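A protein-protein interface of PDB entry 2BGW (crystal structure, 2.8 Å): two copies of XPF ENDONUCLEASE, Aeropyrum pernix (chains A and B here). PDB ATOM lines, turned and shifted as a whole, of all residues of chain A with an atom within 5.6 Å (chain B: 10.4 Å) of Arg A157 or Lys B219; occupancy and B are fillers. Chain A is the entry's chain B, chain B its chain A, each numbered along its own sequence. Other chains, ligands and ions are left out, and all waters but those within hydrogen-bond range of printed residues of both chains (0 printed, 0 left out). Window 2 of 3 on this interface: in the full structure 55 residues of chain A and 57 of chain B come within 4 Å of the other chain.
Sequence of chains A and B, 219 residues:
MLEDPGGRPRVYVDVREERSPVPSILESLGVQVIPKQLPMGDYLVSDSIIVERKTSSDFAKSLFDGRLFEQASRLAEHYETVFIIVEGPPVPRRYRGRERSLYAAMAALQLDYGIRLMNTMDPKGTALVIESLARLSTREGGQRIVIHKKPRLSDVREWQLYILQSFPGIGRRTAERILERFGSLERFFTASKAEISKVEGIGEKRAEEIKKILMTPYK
Among the printed residues, merely in contact across the chains: Arg A157 with Lys B219, Arg A157 with Tyr B218, Trp A159 with Pro B168, Leu A179 with Tyr B218, Gln A160 with Ile B213, Gln A160 with Tyr B218, Val A156 with Thr B216 and Trp A159 with Ile B213.
Val A156 touches just one residue of chain B: Thr B216. Arg A157 touches just these residues of chain B: Tyr B218 and Lys B219. No residue of chain B comes within 4 Å of Glu A158. Of the printed residues of chain B, Trp A159 touches Pro B168 and Ile B213. Of chain B, only Ile B213, Thr B216 and Tyr B218 come within 4 Å of Gln A160. Leu A161 touches none of the printed residues of chain B. Printed residues of chain A within 4 Å of Pro B168: Trp A159 (3.5 Å). Of the printed residues of chain A, Ile B213 touches Trp A159 (3.9 Å) and Gln A160 (3.5 Å). Printed residues of chain A within 4 Å of Thr B216: Val A156 (3.9 Å) and Gln A160 (2.8 Å). Of the printed residues of chain A, Tyr B218 touches Arg A157, Gln A160 and Leu A179. The nearest printed residue of chain B that does not touch Trp A159 is Glu B209 (4.02 Å).
No position is printed for both chains. Of the 9 pairs that touch across the chains among the printed residues, none has its exchanged pair printed and touching as well.
The backbone carbonyl oxygen of Lys B212 lies within hydrogen-bond range of the side-chain hydroxyl of Thr B216, at 3.1 Å.
The backbone carbonyl oxygen (O) of Thr B216 lies within hydrogen-bond range of the side-chain amide nitrogen (NE2) of Gln A160 (2.8 Å).
Hydrophobic or aromatic side chains of chain B that line the printed part of chain A: Pro B168, Ile B213 and Tyr B218. Along chain B the printed residues that touch a printed residue of chain A span positions 168 to 219. Printed residues of chain A that touch a printed residue of chain B: Val A156, Arg A157, Trp A159, Gln A160 and Leu A179. Hydrophobic or aromatic side chains of chain A within 4 Å of the printed part of chain B: Val A156, Trp A159 and Leu A179. Among the printed residues, 9 pairs touch across the chains. Among the printed residues, no Asp or Glu carboxylate lies within 4 Å of a Lys or Arg side-chain nitrogen of the other chain.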
ATOM      1  N   ASP A 155     -23.972   9.068 -29.780  1.00  0.00           N
ATOM      2  CA  ASP A 155     -22.699   8.477 -30.155  1.00  0.00           C
ATOM      3  C   ASP A 155     -21.765   8.630 -28.979  1.00  0.00           C
ATOM      4  O   ASP A 155     -21.519   9.744 -28.489  1.00  0.00           O
ATOM      5  CB  ASP A 155     -22.066   9.138 -31.375  1.00  0.00           C
ATOM      6  CG  ASP A 155     -20.753   8.450 -31.790  1.00  0.00           C
ATOM      7  OD1 ASP A 155     -19.666   9.033 -31.549  1.00  0.00           O
ATOM      8  OD2 ASP A 155     -20.812   7.314 -32.335  1.00  0.00           O
ATOM      9  N   VAL A 156     -21.231   7.498 -28.550  1.00  0.00           N
ATOM     10  CA  VAL A 156     -20.507   7.422 -27.303  1.00  0.00           C
ATOM     11  C   VAL A 156     -19.395   8.445 -27.227  1.00  0.00           C
ATOM     12  O   VAL A 156     -19.352   9.226 -26.292  1.00  0.00           O
ATOM     13  CB  VAL A 156     -20.059   5.995 -27.035  1.00  0.00           C
ATOM     14  CG1 VAL A 156     -19.053   5.940 -25.921  1.00  0.00           C
ATOM     15  CG2 VAL A 156     -21.275   5.155 -26.701  1.00  0.00           C
ATOM     16  N   ARG A 157     -18.528   8.491 -28.222  1.00  0.00           N
ATOM     17  CA  ARG A 157     -17.478   9.525 -28.265  1.00  0.00           C
ATOM     18  C   ARG A 157     -17.921  10.942 -27.778  1.00  0.00           C
ATOM     19  O   ARG A 157     -17.167  11.663 -27.108  1.00  0.00           O
ATOM     20  CB  ARG A 157     -16.856   9.540 -29.681  1.00  0.00           C
ATOM     21  CG  ARG A 157     -16.828  10.898 -30.466  1.00  0.00           C
ATOM     22  CD  ARG A 157     -15.505  11.620 -30.304  1.00  0.00           C
ATOM     23  NE  ARG A 157     -14.434  10.666 -30.524  1.00  0.00           N
ATOM     24  CZ  ARG A 157     -13.510  10.765 -31.473  1.00  0.00           C
ATOM     25  NH1 ARG A 157     -13.490  11.827 -32.283  1.00  0.00           N
ATOM     26  NH2 ARG A 157     -12.587   9.811 -31.584  1.00  0.00           N
ATOM     27  N   GLU A 158     -19.153  11.321 -28.106  1.00  0.00           N
ATOM     28  CA  GLU A 158     -19.648  12.677 -27.837  1.00  0.00           C
ATOM     29  C   GLU A 158     -20.151  12.876 -26.403  1.00  0.00           C
ATOM     30  O   GLU A 158     -19.806  13.854 -25.736  1.00  0.00           O
ATOM     31  CB  GLU A 158     -20.707  13.066 -28.870  1.00  0.00           C
ATOM     32  CG  GLU A 158     -20.095  13.579 -30.193  1.00  0.00           C
ATOM     33  CD  GLU A 158     -19.430  14.986 -30.070  1.00  0.00           C
ATOM     34  OE1 GLU A 158     -19.740  15.750 -29.130  1.00  0.00           O
ATOM     35  OE2 GLU A 158     -18.589  15.345 -30.919  1.00  0.00           O
ATOM     36  N   TRP A 159     -20.941  11.922 -25.926  1.00  0.00           N
ATOM     37  CA  TRP A 159     -21.307  11.870 -24.522  1.00  0.00           C
ATOM     38  C   TRP A 159     -20.090  11.965 -23.615  1.00  0.00           C
ATOM     39  O   TRP A 159     -20.152  12.593 -22.551  1.00  0.00           O
ATOM     40  CB  TRP A 159     -22.067  10.585 -24.225  1.00  0.00           C
ATOM     41  CG  TRP A 159     -23.463  10.610 -24.723  1.00  0.00           C
ATOM     42  CD1 TRP A 159     -23.969   9.894 -25.750  1.00  0.00           C
ATOM     43  CD2 TRP A 159     -24.532  11.397 -24.214  1.00  0.00           C
ATOM     44  NE1 TRP A 159     -25.299  10.172 -25.919  1.00  0.00           N
ATOM     45  CE2 TRP A 159     -25.673  11.097 -24.986  1.00  0.00           C
ATOM     46  CE3 TRP A 159     -24.641  12.331 -23.178  1.00  0.00           C
ATOM     47  CZ2 TRP A 159     -26.918  11.694 -24.759  1.00  0.00           C
ATOM     48  CZ3 TRP A 159     -25.886  12.931 -22.946  1.00  0.00           C
ATOM     49  CH2 TRP A 159     -27.007  12.605 -23.733  1.00  0.00           C
ATOM     50  N   GLN A 160     -18.992  11.347 -24.048  1.00  0.00           N
ATOM     51  CA  GLN A 160     -17.748  11.363 -23.303  1.00  0.00           C
ATOM     52  C   GLN A 160     -17.222  12.773 -23.175  1.00  0.00           C
ATOM     53  O   GLN A 160     -16.854  13.194 -22.073  1.00  0.00           O
ATOM     54  CB  GLN A 160     -16.699  10.491 -23.976  1.00  0.00           C
ATOM     55  CG  GLN A 160     -16.900   9.014 -23.779  1.00  0.00           C
ATOM     56  CD  GLN A 160     -16.084   8.153 -24.741  1.00  0.00           C
ATOM     57  OE1 GLN A 160     -15.448   8.647 -25.689  1.00  0.00           O
ATOM     58  NE2 GLN A 160     -16.114   6.844 -24.507  1.00  0.00           N
ATOM     59  N   LEU A 161     -17.180  13.514 -24.283  1.00  0.00           N
ATOM     60  CA  LEU A 161     -16.616  14.865 -24.227  1.00  0.00           C
ATOM     61  C   LEU A 161     -17.526  15.841 -23.460  1.00  0.00           C
ATOM     62  O   LEU A 161     -17.050  16.770 -22.788  1.00  0.00           O
ATOM     63  CB  LEU A 161     -16.310  15.376 -25.625  1.00  0.00           C
ATOM     64  CG  LEU A 161     -15.167  14.692 -26.368  1.00  0.00           C
ATOM     65  CD1 LEU A 161     -15.269  14.990 -27.849  1.00  0.00           C
ATOM     66  CD2 LEU A 161     -13.825  15.151 -25.847  1.00  0.00           C
ATOM     67  N   TYR A 162     -18.829  15.598 -23.563  1.00  0.00           N
ATOM     68  CA  TYR A 162     -19.831  16.297 -22.782  1.00  0.00           C
ATOM     69  C   TYR A 162     -19.661  16.151 -21.251  1.00  0.00           C
ATOM     70  O   TYR A 162     -19.588  17.157 -20.503  1.00  0.00           O
ATOM     71  CB  TYR A 162     -21.210  15.792 -23.196  1.00  0.00           C
ATOM     72  CG  TYR A 162     -22.382  16.599 -22.645  1.00  0.00           C
ATOM     73  CD1 TYR A 162     -22.552  17.947 -22.982  1.00  0.00           C
ATOM     74  CD2 TYR A 162     -23.331  16.004 -21.804  1.00  0.00           C
ATOM     75  CE1 TYR A 162     -23.611  18.678 -22.487  1.00  0.00           C
ATOM     76  CE2 TYR A 162     -24.406  16.735 -21.313  1.00  0.00           C
ATOM     77  CZ  TYR A 162     -24.539  18.071 -21.660  1.00  0.00           C
ATOM     78  OH  TYR A 162     -25.602  18.800 -21.178  1.00  0.00           O
ATOM     79  N   LEU A 179      -9.075  12.498 -23.004  1.00  0.00           N
ATOM     80  CA  LEU A 179      -9.416  11.228 -23.608  1.00  0.00           C
ATOM     81  C   LEU A 179      -8.285  10.645 -24.485  1.00  0.00           C
ATOM     82  O   LEU A 179      -8.127   9.416 -24.588  1.00  0.00           O
ATOM     83  CB  LEU A 179     -10.733  11.342 -24.352  1.00  0.00           C
ATOM     84  CG  LEU A 179     -11.923  11.238 -23.411  1.00  0.00           C
ATOM     85  CD1 LEU A 179     -13.185  11.575 -24.157  1.00  0.00           C
ATOM     86  CD2 LEU A 179     -12.025   9.863 -22.806  1.00  0.00           C
ATOM     87  N   PRO B 168     -26.941  10.221 -19.984  1.00  0.00           N
ATOM     88  CA  PRO B 168     -28.257   9.917 -20.514  1.00  0.00           C
ATOM     89  C   PRO B 168     -28.988   9.086 -19.474  1.00  0.00           C
ATOM     90  O   PRO B 168     -28.333   8.365 -18.745  1.00  0.00           O
ATOM     91  CB  PRO B 168     -27.939   9.059 -21.732  1.00  0.00           C
ATOM     92  CG  PRO B 168     -26.536   9.407 -22.077  1.00  0.00           C
ATOM     93  CD  PRO B 168     -25.882   9.586 -20.786  1.00  0.00           C
ATOM     94  N   GLU B 209     -26.097   1.568 -21.464  1.00  0.00           N
ATOM     95  CA  GLU B 209     -25.673   2.842 -22.026  1.00  0.00           C
ATOM     96  C   GLU B 209     -24.558   3.491 -21.167  1.00  0.00           C
ATOM     97  O   GLU B 209     -23.542   3.994 -21.698  1.00  0.00           O
ATOM     98  CB  GLU B 209     -26.899   3.762 -22.217  1.00  0.00           C
ATOM     99  CG  GLU B 209     -26.624   5.228 -22.638  1.00  0.00           C
ATOM    100  CD  GLU B 209     -26.038   5.361 -24.033  1.00  0.00           C
ATOM    101  OE1 GLU B 209     -25.463   4.378 -24.548  1.00  0.00           O
ATOM    102  OE2 GLU B 209     -26.142   6.454 -24.632  1.00  0.00           O
ATOM    103  N   LYS B 212     -21.333   1.370 -21.215  1.00  0.00           N
ATOM    104  CA  LYS B 212     -20.713   1.530 -22.525  1.00  0.00           C
ATOM    105  C   LYS B 212     -20.013   2.876 -22.577  1.00  0.00           C
ATOM    106  O   LYS B 212     -18.893   2.950 -23.071  1.00  0.00           O
ATOM    107  CB  LYS B 212     -21.693   1.341 -23.695  1.00  0.00           C
ATOM    108  N   ILE B 213     -20.620   3.930 -22.027  1.00  0.00           N
ATOM    109  CA  ILE B 213     -19.946   5.243 -22.027  1.00  0.00           C
ATOM    110  C   ILE B 213     -18.686   5.280 -21.146  1.00  0.00           C
ATOM    111  O   ILE B 213     -17.679   5.886 -21.504  1.00  0.00           O
ATOM    112  CB  ILE B 213     -20.877   6.372 -21.612  1.00  0.00           C
ATOM    113  CG1 ILE B 213     -21.870   6.659 -22.720  1.00  0.00           C
ATOM    114  CG2 ILE B 213     -20.074   7.639 -21.334  1.00  0.00           C
ATOM    115  CD1 ILE B 213     -23.102   7.371 -22.235  1.00  0.00           C
ATOM    116  N   LEU B 214     -18.760   4.624 -19.998  1.00  0.00           N
ATOM    117  CA  LEU B 214     -17.689   4.643 -19.049  1.00  0.00           C
ATOM    118  C   LEU B 214     -16.465   3.935 -19.585  1.00  0.00           C
ATOM    119  O   LEU B 214     -15.343   4.252 -19.189  1.00  0.00           O
ATOM    120  CB  LEU B 214     -18.153   3.958 -17.777  1.00  0.00           C
ATOM    121  CG  LEU B 214     -19.071   4.771 -16.873  1.00  0.00           C
ATOM    122  CD1 LEU B 214     -19.732   3.882 -15.852  1.00  0.00           C
ATOM    123  CD2 LEU B 214     -18.281   5.896 -16.196  1.00  0.00           C
ATOM    124  N   MET B 215     -16.683   2.992 -20.506  1.00  0.00           N
ATOM    125  CA  MET B 215     -15.645   2.023 -20.915  1.00  0.00           C
ATOM    126  C   MET B 215     -15.180   2.085 -22.360  1.00  0.00           C
ATOM    127  O   MET B 215     -14.030   1.785 -22.635  1.00  0.00           O
ATOM    128  CB  MET B 215     -16.092   0.599 -20.633  1.00  0.00           C
ATOM    129  CG  MET B 215     -16.595   0.398 -19.230  1.00  0.00           C
ATOM    130  SD  MET B 215     -16.187  -1.233 -18.581  1.00  0.00           S
ATOM    131  CE  MET B 215     -14.357  -1.183 -18.560  1.00  0.00           C
ATOM    132  N   THR B 216     -16.046   2.448 -23.292  1.00  0.00           N
ATOM    133  CA  THR B 216     -15.635   2.446 -24.687  1.00  0.00           C
ATOM    134  C   THR B 216     -14.430   3.365 -24.963  1.00  0.00           C
ATOM    135  O   THR B 216     -14.531   4.562 -24.814  1.00  0.00           O
ATOM    136  CB  THR B 216     -16.810   2.742 -25.613  1.00  0.00           C
ATOM    137  OG1 THR B 216     -17.690   1.610 -25.621  1.00  0.00           O
ATOM    138  CG2 THR B 216     -16.315   2.979 -27.019  1.00  0.00           C
ATOM    139  N   PRO B 217     -13.275   2.781 -25.344  1.00  0.00           N
ATOM    140  CA  PRO B 217     -12.053   3.526 -25.657  1.00  0.00           C
ATOM    141  C   PRO B 217     -12.236   4.624 -26.682  1.00  0.00           C
ATOM    142  O   PRO B 217     -13.120   4.569 -27.509  1.00  0.00           O
ATOM    143  CB  PRO B 217     -11.103   2.458 -26.218  1.00  0.00           C
ATOM    144  CG  PRO B 217     -11.908   1.258 -26.416  1.00  0.00           C
ATOM    145  CD  PRO B 217     -13.054   1.328 -25.473  1.00  0.00           C
ATOM    146  N   TYR B 218     -11.375   5.612 -26.623  1.00  0.00           N
ATOM    147  CA  TYR B 218     -11.556   6.782 -27.401  1.00  0.00           C
ATOM    148  C   TYR B 218     -10.558   6.760 -28.542  1.00  0.00           C
ATOM    149  O   TYR B 218      -9.364   6.961 -28.325  1.00  0.00           O
ATOM    150  CB  TYR B 218     -11.345   7.987 -26.490  1.00  0.00           C
ATOM    151  CG  TYR B 218     -11.309   9.341 -27.172  1.00  0.00           C
ATOM    152  CD1 TYR B 218     -12.492  10.031 -27.484  1.00  0.00           C
ATOM    153  CD2 TYR B 218     -10.082   9.951 -27.474  1.00  0.00           C
ATOM    154  CE1 TYR B 218     -12.449  11.282 -28.091  1.00  0.00           C
ATOM    155  CE2 TYR B 218     -10.029  11.202 -28.088  1.00  0.00           C
ATOM    156  CZ  TYR B 218     -11.214  11.861 -28.399  1.00  0.00           C
ATOM    157  OH  TYR B 218     -11.133  13.093 -29.009  1.00  0.00           O
ATOM    158  N   LYS B 219     -11.052   6.505 -29.755  1.00  0.00           N
ATOM    159  CA  LYS B 219     -10.275   6.644 -31.009  1.00  0.00           C
ATOM    160  C   LYS B 219     -10.006   8.128 -31.387  1.00  0.00           C
ATOM    161  O   LYS B 219      -8.861   8.625 -31.389  1.00  0.00           O
ATOM    162  CB  LYS B 219     -11.020   5.942 -32.160  1.00  0.00           C
